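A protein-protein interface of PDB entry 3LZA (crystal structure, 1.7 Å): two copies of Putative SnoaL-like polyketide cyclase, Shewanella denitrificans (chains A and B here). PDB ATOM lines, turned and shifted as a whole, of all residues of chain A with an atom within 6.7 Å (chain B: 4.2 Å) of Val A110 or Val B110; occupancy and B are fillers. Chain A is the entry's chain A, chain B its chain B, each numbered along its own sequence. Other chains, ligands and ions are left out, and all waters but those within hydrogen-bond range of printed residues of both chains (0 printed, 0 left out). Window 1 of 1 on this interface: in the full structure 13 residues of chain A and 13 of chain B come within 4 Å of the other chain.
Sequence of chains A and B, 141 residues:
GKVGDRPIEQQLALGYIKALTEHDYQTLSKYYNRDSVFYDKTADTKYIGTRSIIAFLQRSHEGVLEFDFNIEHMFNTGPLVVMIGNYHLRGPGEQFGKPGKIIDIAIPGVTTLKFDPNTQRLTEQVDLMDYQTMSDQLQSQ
The backbone NH (N) of Val A82 lies within hydrogen-bond range of the backbone carbonyl oxygen (O) of Phe A75, at 2.8 Å.
O of Val A110 sits at hydrogen-bond distance from N of Leu A128.
The backbone NH (N) of Thr A112 lies within hydrogen-bond range of the backbone carbonyl oxygen (O) of Val A126 (2.8 Å).
The backbone carbonyl oxygen of Leu B128 sits at hydrogen-bond distance from the backbone NH of Val B110 (2.9 Å).
Of the 18 printed residues of chain A, 4 touch a printed residue of chain B.
Hydrophobic or aromatic side chains of chain A that line the printed part of chain B: Phe A75, Ile A84 and Val A110.
Hydrophobic or aromatic side chains of chain B within 4 Å of the printed part of chain A: Ile B84, Val B110 and Leu B128.
Among the printed residues, no Asp or Glu carboxylate lies within 4 Å of a Lys or Arg side-chain nitrogen of the other chain.
Val A110 touches just these residues of chain B: Ile B84 and Val B110.
Val B110 touches just these residues of chain A: Ile A84 (3.9 Å) and Val A110 (3.9 Å).
Of the printed residues of chain A, Ile B84 touches Ile A84 (3.7 Å) and Val A110 (3.6 Å).
Printed residues of chain B within 4 Å of Phe A75: Leu B128 (3.8 Å) and Met B129 (3.5 Å).
Gly A85 touches none of the printed residues of chain B.
Thr A111 touches none of the printed residues of chain B.
The nearest printed residue of chain B that does not touch Val A110 is Val B82 (4.8 Å).
The nearest residue of chain A that does not touch Val B110 is Leu A128 (4.7 Å).
Leu B128 touches Phe A75 (O to CZ, 3.8 Å).
C of Met B129 touches CE2 of Phe A75, at 3.5 Å.
Ile B84 touches Ile A84.
Val B110 touches Ile A84 (CG2 to CD1, 3.9 Å).
CG2 of Val A110 touches CD1 of Ile B84, at 3.6 Å.
CG2 of Val A110 touches CG2 of Val B110 (3.9 Å).
CG2 of Thr A112 touches CD1 of Leu B128 (3.6 Å).
Ile A84 touches its own counterpart, Ile B84.
Ile A84 touches Val B110, and with the chains exchanged Val A110 touches Ile B84.
Val A110 touches its own counterpart, Val B110.
Positions printed for both chains: 82, 83, 84, 109, 110, 111, 126, 127, 128 and 129.
Of the 7 pairs that touch across the chains among the printed residues, 4 have their exchanged pair printed and touching as well.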
ATOM      1  N   PHE A  69      13.240  -7.323 -25.590  1.00  0.00           N
ATOM      2  CA  PHE A  69      12.381  -6.150 -25.720  1.00  0.00           C
ATOM      3  C   PHE A  69      11.421  -6.454 -26.859  1.00  0.00           C
ATOM      4  O   PHE A  69      11.781  -6.463 -28.083  1.00  0.00           O
ATOM      5  CB  PHE A  69      13.232  -4.894 -25.994  1.00  0.00           C
ATOM      6  CG  PHE A  69      12.458  -3.578 -26.063  1.00  0.00           C
ATOM      7  CD1 PHE A  69      11.205  -3.411 -25.462  1.00  0.00           C
ATOM      8  CD2 PHE A  69      13.028  -2.497 -26.706  1.00  0.00           C
ATOM      9  CE1 PHE A  69      10.512  -2.174 -25.540  1.00  0.00           C
ATOM     10  CE2 PHE A  69      12.347  -1.222 -26.782  1.00  0.00           C
ATOM     11  CZ  PHE A  69      11.087  -1.077 -26.172  1.00  0.00           C
ATOM     12  N   PHE A  75       8.927   4.065 -34.304  1.00  0.00           N
ATOM     13  CA  PHE A  75       8.927   5.143 -35.282  1.00  0.00           C
ATOM     14  C   PHE A  75      10.085   6.084 -35.073  1.00  0.00           C
ATOM     15  O   PHE A  75      10.758   5.983 -34.072  1.00  0.00           O
ATOM     16  CB  PHE A  75       7.602   5.935 -35.254  1.00  0.00           C
ATOM     17  CG  PHE A  75       7.188   6.461 -33.905  1.00  0.00           C
ATOM     18  CD1 PHE A  75       6.455   5.693 -33.008  1.00  0.00           C
ATOM     19  CD2 PHE A  75       7.459   7.774 -33.562  1.00  0.00           C
ATOM     20  CE1 PHE A  75       6.009   6.254 -31.791  1.00  0.00           C
ATOM     21  CE2 PHE A  75       7.043   8.316 -32.362  1.00  0.00           C
ATOM     22  CZ  PHE A  75       6.312   7.551 -31.482  1.00  0.00           C
ATOM     23  N   VAL A  82      11.837   5.970 -31.482  1.00  0.00           N
ATOM     24  CA  VAL A  82      10.957   5.706 -30.323  1.00  0.00           C
ATOM     25  C   VAL A  82      10.398   4.296 -30.421  1.00  0.00           C
ATOM     26  O   VAL A  82       9.876   3.907 -31.460  1.00  0.00           O
ATOM     27  CB  VAL A  82       9.743   6.726 -30.283  1.00  0.00           C
ATOM     28  CG1 VAL A  82       8.818   6.459 -29.077  1.00  0.00           C
ATOM     29  CG2 VAL A  82      10.244   8.130 -30.225  1.00  0.00           C
ATOM     30  N   MET A  83      10.459   3.560 -29.324  1.00  0.00           N
ATOM     31  CA  MET A  83      10.058   2.164 -29.314  1.00  0.00           C
ATOM     32  C   MET A  83       9.134   1.888 -28.131  1.00  0.00           C
ATOM     33  O   MET A  83       9.471   2.190 -27.011  1.00  0.00           O
ATOM     34  CB  MET A  83      11.343   1.309 -29.231  1.00  0.00           C
ATOM     35  CG  MET A  83      12.147   1.386 -30.490  1.00  0.00           C
ATOM     36  SD  MET A  83      13.885   0.586 -30.264  1.00  0.00           S
ATOM     37  CE  MET A  83      14.596   1.884 -29.131  1.00  0.00           C
ATOM     38  N   ILE A  84       7.926   1.391 -28.423  1.00  0.00           N
ATOM     39  CA  ILE A  84       6.899   1.092 -27.427  1.00  0.00           C
ATOM     40  C   ILE A  84       6.727  -0.413 -27.323  1.00  0.00           C
ATOM     41  O   ILE A  84       6.614  -1.094 -28.326  1.00  0.00           O
ATOM     42  CB  ILE A  84       5.532   1.702 -27.826  1.00  0.00           C
ATOM     43  CG1 ILE A  84       5.643   3.217 -28.009  1.00  0.00           C
ATOM     44  CG2 ILE A  84       4.429   1.328 -26.803  1.00  0.00           C
ATOM     45  CD1 ILE A  84       4.641   3.779 -28.933  1.00  0.00           C
ATOM     46  N   GLY A  85       6.743  -0.939 -26.101  1.00  0.00           N
ATOM     47  CA  GLY A  85       6.562  -2.355 -25.918  1.00  0.00           C
ATOM     48  C   GLY A  85       6.663  -2.829 -24.487  1.00  0.00           C
ATOM     49  O   GLY A  85       6.221  -2.159 -23.558  1.00  0.00           O
ATOM     50  N   TYR A  87       9.476  -5.232 -21.865  1.00  0.00           N
ATOM     51  CA  TYR A  87      10.690  -5.967 -21.623  1.00  0.00           C
ATOM     52  C   TYR A  87      10.357  -7.224 -20.817  1.00  0.00           C
ATOM     53  O   TYR A  87       9.784  -7.138 -19.724  1.00  0.00           O
ATOM     54  CB  TYR A  87      11.627  -5.071 -20.814  1.00  0.00           C
ATOM     55  CG  TYR A  87      12.333  -4.013 -21.629  1.00  0.00           C
ATOM     56  CD1 TYR A  87      11.746  -2.763 -21.853  1.00  0.00           C
ATOM     57  CD2 TYR A  87      13.626  -4.235 -22.129  1.00  0.00           C
ATOM     58  CE1 TYR A  87      12.415  -1.787 -22.587  1.00  0.00           C
ATOM     59  CE2 TYR A  87      14.297  -3.244 -22.881  1.00  0.00           C
ATOM     60  CZ  TYR A  87      13.690  -2.018 -23.069  1.00  0.00           C
ATOM     61  OH  TYR A  87      14.354  -1.037 -23.781  1.00  0.00           O
ATOM     62  N   ILE A 107       7.598  -6.167 -18.293  1.00  0.00           N
ATOM     63  CA  ILE A 107       7.549  -4.754 -17.891  1.00  0.00           C
ATOM     64  C   ILE A 107       7.196  -3.839 -19.067  1.00  0.00           C
ATOM     65  O   ILE A 107       8.001  -3.695 -19.980  1.00  0.00           O
ATOM     66  CB  ILE A 107       8.947  -4.283 -17.358  1.00  0.00           C
ATOM     67  CG1 ILE A 107       9.563  -5.282 -16.375  1.00  0.00           C
ATOM     68  CG2 ILE A 107       8.847  -2.909 -16.663  1.00  0.00           C
ATOM     69  CD1 ILE A 107      10.830  -4.767 -15.742  1.00  0.00           C
ATOM     70  N   PRO A 108       6.019  -3.181 -19.039  1.00  0.00           N
ATOM     71  CA  PRO A 108       5.757  -2.209 -20.114  1.00  0.00           C
ATOM     72  C   PRO A 108       6.788  -1.108 -20.096  1.00  0.00           C
ATOM     73  O   PRO A 108       7.185  -0.658 -19.033  1.00  0.00           O
ATOM     74  CB  PRO A 108       4.428  -1.609 -19.693  1.00  0.00           C
ATOM     75  CG  PRO A 108       3.740  -2.782 -19.028  1.00  0.00           C
ATOM     76  CD  PRO A 108       4.818  -3.430 -18.239  1.00  0.00           C
ATOM     77  N   GLY A 109       7.202  -0.636 -21.247  1.00  0.00           N
ATOM     78  CA  GLY A 109       8.093   0.460 -21.233  1.00  0.00           C
ATOM     79  C   GLY A 109       8.156   1.162 -22.580  1.00  0.00           C
ATOM     80  O   GLY A 109       7.694   0.641 -23.615  1.00  0.00           O
ATOM     81  N   VAL A 110       8.648   2.377 -22.522  1.00  0.00           N
ATOM     82  CA  VAL A 110       8.977   3.173 -23.749  1.00  0.00           C
ATOM     83  C   VAL A 110      10.460   3.548 -23.708  1.00  0.00           C
ATOM     84  O   VAL A 110      10.904   4.103 -22.725  1.00  0.00           O
ATOM     85  CB  VAL A 110       8.077   4.436 -23.863  1.00  0.00           C
ATOM     86  CG1 VAL A 110       8.421   5.282 -25.064  1.00  0.00           C
ATOM     87  CG2 VAL A 110       6.604   3.999 -24.006  1.00  0.00           C
ATOM     88  N   THR A 111      11.188   3.242 -24.781  1.00  0.00           N
ATOM     89  CA  THR A 111      12.623   3.550 -24.914  1.00  0.00           C
ATOM     90  C   THR A 111      12.834   4.494 -26.118  1.00  0.00           C
ATOM     91  O   THR A 111      12.365   4.200 -27.238  1.00  0.00           O
ATOM     92  CB  THR A 111      13.451   2.181 -25.043  1.00  0.00           C
ATOM     93  OG1 THR A 111      13.306   1.471 -23.807  1.00  0.00           O
ATOM     94  CG2 THR A 111      14.938   2.429 -25.306  1.00  0.00           C
ATOM     95  N   THR A 112      13.546   5.617 -25.926  1.00  0.00           N
ATOM     96  CA  THR A 112      14.041   6.416 -27.055  1.00  0.00           C
ATOM     97  C   THR A 112      15.552   6.281 -27.184  1.00  0.00           C
ATOM     98  O   THR A 112      16.254   6.162 -26.179  1.00  0.00           O
ATOM     99  CB  THR A 112      13.646   7.938 -26.939  1.00  0.00           C
ATOM    100  OG1 THR A 112      14.358   8.564 -25.870  1.00  0.00           O
ATOM    101  CG2 THR A 112      12.127   8.053 -26.669  1.00  0.00           C
ATOM    102  N   VAL A 126      16.792   7.006 -23.470  1.00  0.00           N
ATOM    103  CA  VAL A 126      15.880   7.327 -22.379  1.00  0.00           C
ATOM    104  C   VAL A 126      14.863   6.197 -22.214  1.00  0.00           C
ATOM    105  O   VAL A 126      14.157   5.821 -23.154  1.00  0.00           O
ATOM    106  CB  VAL A 126      15.155   8.672 -22.496  1.00  0.00           C
ATOM    107  CG1 VAL A 126      14.388   8.915 -21.147  1.00  0.00           C
ATOM    108  CG2 VAL A 126      16.164   9.824 -22.738  1.00  0.00           C
ATOM    109  N   ASP A 127      14.830   5.636 -21.004  1.00  0.00           N
ATOM    110  CA  ASP A 127      13.870   4.600 -20.670  1.00  0.00           C
ATOM    111  C   ASP A 127      12.806   5.159 -19.789  1.00  0.00           C
ATOM    112  O   ASP A 127      13.097   5.903 -18.857  1.00  0.00           O
ATOM    113  CB  ASP A 127      14.519   3.394 -19.963  1.00  0.00           C
ATOM    114  CG  ASP A 127      15.278   2.489 -20.877  1.00  0.00           C
ATOM    115  OD1 ASP A 127      15.263   2.647 -22.139  1.00  0.00           O
ATOM    116  OD2 ASP A 127      15.943   1.601 -20.308  1.00  0.00           O
ATOM    117  N   LEU A 128      11.551   4.801 -20.087  1.00  0.00           N
ATOM    118  CA  LEU A 128      10.432   5.059 -19.185  1.00  0.00           C
ATOM    119  C   LEU A 128       9.805   3.679 -18.901  1.00  0.00           C
ATOM    120  O   LEU A 128       9.221   3.076 -19.783  1.00  0.00           O
ATOM    121  CB  LEU A 128       9.400   6.012 -19.835  1.00  0.00           C
ATOM    122  CG  LEU A 128       9.802   7.453 -20.191  1.00  0.00           C
ATOM    123  CD1 LEU A 128       8.910   8.061 -21.271  1.00  0.00           C
ATOM    124  CD2 LEU A 128       9.757   8.296 -18.923  1.00  0.00           C
ATOM    125  N   MET A 129       9.953   3.157 -17.675  1.00  0.00           N
ATOM    126  CA  MET A 129       9.573   1.796 -17.361  1.00  0.00           C
ATOM    127  C   MET A 129       8.440   1.786 -16.374  1.00  0.00           C
ATOM    128  O   MET A 129       8.397   2.610 -15.443  1.00  0.00           O
ATOM    129  CB  MET A 129      10.750   1.018 -16.782  1.00  0.00           C
ATOM    130  CG  MET A 129      11.999   0.993 -17.610  1.00  0.00           C
ATOM    131  SD  MET A 129      11.722  -0.187 -19.144  1.00  0.00           S
ATOM    132  CE  MET A 129      11.359  -1.767 -18.210  1.00  0.00           C
ATOM    133  N   ASP A 130       7.502   0.851 -16.556  1.00  0.00           N
ATOM    134  CA  ASP A 130       6.374   0.699 -15.637  1.00  0.00           C
ATOM    135  C   ASP A 130       6.777  -0.169 -14.418  1.00  0.00           C
ATOM    136  O   ASP A 130       6.484  -1.369 -14.349  1.00  0.00           O
ATOM    137  CB  ASP A 130       5.170   0.122 -16.388  1.00  0.00           C
ATOM    138  CG  ASP A 130       3.937  -0.066 -15.551  1.00  0.00           C
ATOM    139  OD1 ASP A 130       3.871   0.307 -14.353  1.00  0.00           O
ATOM    140  OD2 ASP A 130       2.988  -0.658 -16.113  1.00  0.00           O
ATOM    141  N   VAL B  82       3.167   8.523 -17.472  1.00  0.00           N
ATOM    142  CA  VAL B  82       3.447   8.129 -18.888  1.00  0.00           C
ATOM    143  C   VAL B  82       2.176   7.581 -19.485  1.00  0.00           C
ATOM    144  O   VAL B  82       1.501   6.755 -18.892  1.00  0.00           O
ATOM    145  CB  VAL B  82       4.568   7.056 -18.962  1.00  0.00           C
ATOM    146  CG1 VAL B  82       4.882   6.674 -20.440  1.00  0.00           C
ATOM    147  CG2 VAL B  82       5.841   7.571 -18.268  1.00  0.00           C
ATOM    148  N   MET B  83       1.791   8.088 -20.645  1.00  0.00           N
ATOM    149  CA  MET B  83       0.579   7.606 -21.306  1.00  0.00           C
ATOM    150  C   MET B  83       0.947   7.209 -22.730  1.00  0.00           C
ATOM    151  O   MET B  83       1.523   7.988 -23.503  1.00  0.00           O
ATOM    152  CB  MET B  83      -0.496   8.705 -21.334  1.00  0.00           C
ATOM    153  CG  MET B  83      -1.055   9.012 -19.950  1.00  0.00           C
ATOM    154  SD  MET B  83      -1.978  10.671 -20.060  1.00  0.00           S
ATOM    155  CE  MET B  83      -0.403  11.572 -19.972  1.00  0.00           C
ATOM    156  N   ILE B  84       0.600   5.974 -23.064  1.00  0.00           N
ATOM    157  CA  ILE B  84       0.830   5.420 -24.386  1.00  0.00           C
ATOM    158  C   ILE B  84      -0.477   5.269 -25.117  1.00  0.00           C
ATOM    159  O   ILE B  84      -1.394   4.682 -24.617  1.00  0.00           O
ATOM    160  CB  ILE B  84       1.446   3.994 -24.237  1.00  0.00           C
ATOM    161  CG1 ILE B  84       2.822   4.069 -23.602  1.00  0.00           C
ATOM    162  CG2 ILE B  84       1.516   3.267 -25.588  1.00  0.00           C
ATOM    163  CD1 ILE B  84       3.359   2.710 -23.071  1.00  0.00           C
ATOM    164  N   GLY B 109       1.261   7.897 -30.263  1.00  0.00           N
ATOM    165  CA  GLY B 109       2.107   8.833 -29.532  1.00  0.00           C
ATOM    166  C   GLY B 109       2.306   8.405 -28.114  1.00  0.00           C
ATOM    167  O   GLY B 109       1.587   7.567 -27.652  1.00  0.00           O
ATOM    168  N   VAL B 110       3.360   8.907 -27.476  1.00  0.00           N
ATOM    169  CA  VAL B 110       3.567   8.752 -26.014  1.00  0.00           C
ATOM    170  C   VAL B 110       3.639  10.172 -25.446  1.00  0.00           C
ATOM    171  O   VAL B 110       4.405  10.983 -25.952  1.00  0.00           O
ATOM    172  CB  VAL B 110       4.886   8.004 -25.731  1.00  0.00           C
ATOM    173  CG1 VAL B 110       5.199   7.998 -24.230  1.00  0.00           C
ATOM    174  CG2 VAL B 110       4.828   6.584 -26.273  1.00  0.00           C
ATOM    175  N   THR B 111       2.864  10.461 -24.402  1.00  0.00           N
ATOM    176  CA  THR B 111       2.836  11.762 -23.762  1.00  0.00           C
ATOM    177  C   THR B 111       3.234  11.507 -22.319  1.00  0.00           C
ATOM    178  O   THR B 111       2.717  10.591 -21.697  1.00  0.00           O
ATOM    179  CB  THR B 111       1.435  12.414 -23.880  1.00  0.00           C
ATOM    180  OG1 THR B 111       1.243  12.888 -25.232  1.00  0.00           O
ATOM    181  CG2 THR B 111       1.270  13.580 -22.954  1.00  0.00           C
ATOM    182  N   VAL B 126       5.653  16.354 -22.252  1.00  0.00           N
ATOM    183  CA  VAL B 126       6.518  16.036 -23.370  1.00  0.00           C
ATOM    184  C   VAL B 126       5.766  15.126 -24.319  1.00  0.00           C
ATOM    185  O   VAL B 126       5.217  14.127 -23.884  1.00  0.00           O
ATOM    186  CB  VAL B 126       7.874  15.362 -22.941  1.00  0.00           C
ATOM    187  CG1 VAL B 126       8.729  15.087 -24.204  1.00  0.00           C
ATOM    188  CG2 VAL B 126       8.650  16.277 -21.957  1.00  0.00           C
ATOM    189  N   ASP B 127       5.737  15.473 -25.610  1.00  0.00           N
ATOM    190  CA  ASP B 127       5.124  14.618 -26.608  1.00  0.00           C
ATOM    191  C   ASP B 127       6.152  13.963 -27.502  1.00  0.00           C
ATOM    192  O   ASP B 127       7.156  14.593 -27.939  1.00  0.00           O
ATOM    193  CB  ASP B 127       4.152  15.414 -27.490  1.00  0.00           C
ATOM    194  CG  ASP B 127       2.812  15.699 -26.810  1.00  0.00           C
ATOM    195  OD1 ASP B 127       2.543  15.228 -25.671  1.00  0.00           O
ATOM    196  OD2 ASP B 127       2.033  16.432 -27.441  1.00  0.00           O
ATOM    197  N   LEU B 128       5.875  12.700 -27.798  1.00  0.00           N
ATOM    198  CA  LEU B 128       6.567  11.939 -28.834  1.00  0.00           C
ATOM    199  C   LEU B 128       5.526  11.408 -29.796  1.00  0.00           C
ATOM    200  O   LEU B 128       4.818  10.441 -29.475  1.00  0.00           O
ATOM    201  CB  LEU B 128       7.321  10.756 -28.183  1.00  0.00           C
ATOM    202  CG  LEU B 128       8.496  11.101 -27.247  1.00  0.00           C
ATOM    203  CD1 LEU B 128       8.990   9.884 -26.490  1.00  0.00           C
ATOM    204  CD2 LEU B 128       9.638  11.739 -28.042  1.00  0.00           C
ATOM    205  N   MET B 129       5.470  11.983 -30.997  1.00  0.00           N
ATOM    206  CA  MET B 129       4.375  11.709 -31.909  1.00  0.00           C
ATOM    207  C   MET B 129       4.952  11.059 -33.147  1.00  0.00           C
ATOM    208  O   MET B 129       5.992  11.497 -33.674  1.00  0.00           O
ATOM    209  CB  MET B 129       3.658  13.003 -32.343  1.00  0.00           C
ATOM    210  CG  MET B 129       3.051  13.830 -31.273  1.00  0.00           C
ATOM    211  SD  MET B 129       1.449  12.901 -30.610  1.00  0.00           S
ATOM    212  CE  MET B 129       2.031  12.738 -28.818  1.00  0.00           C
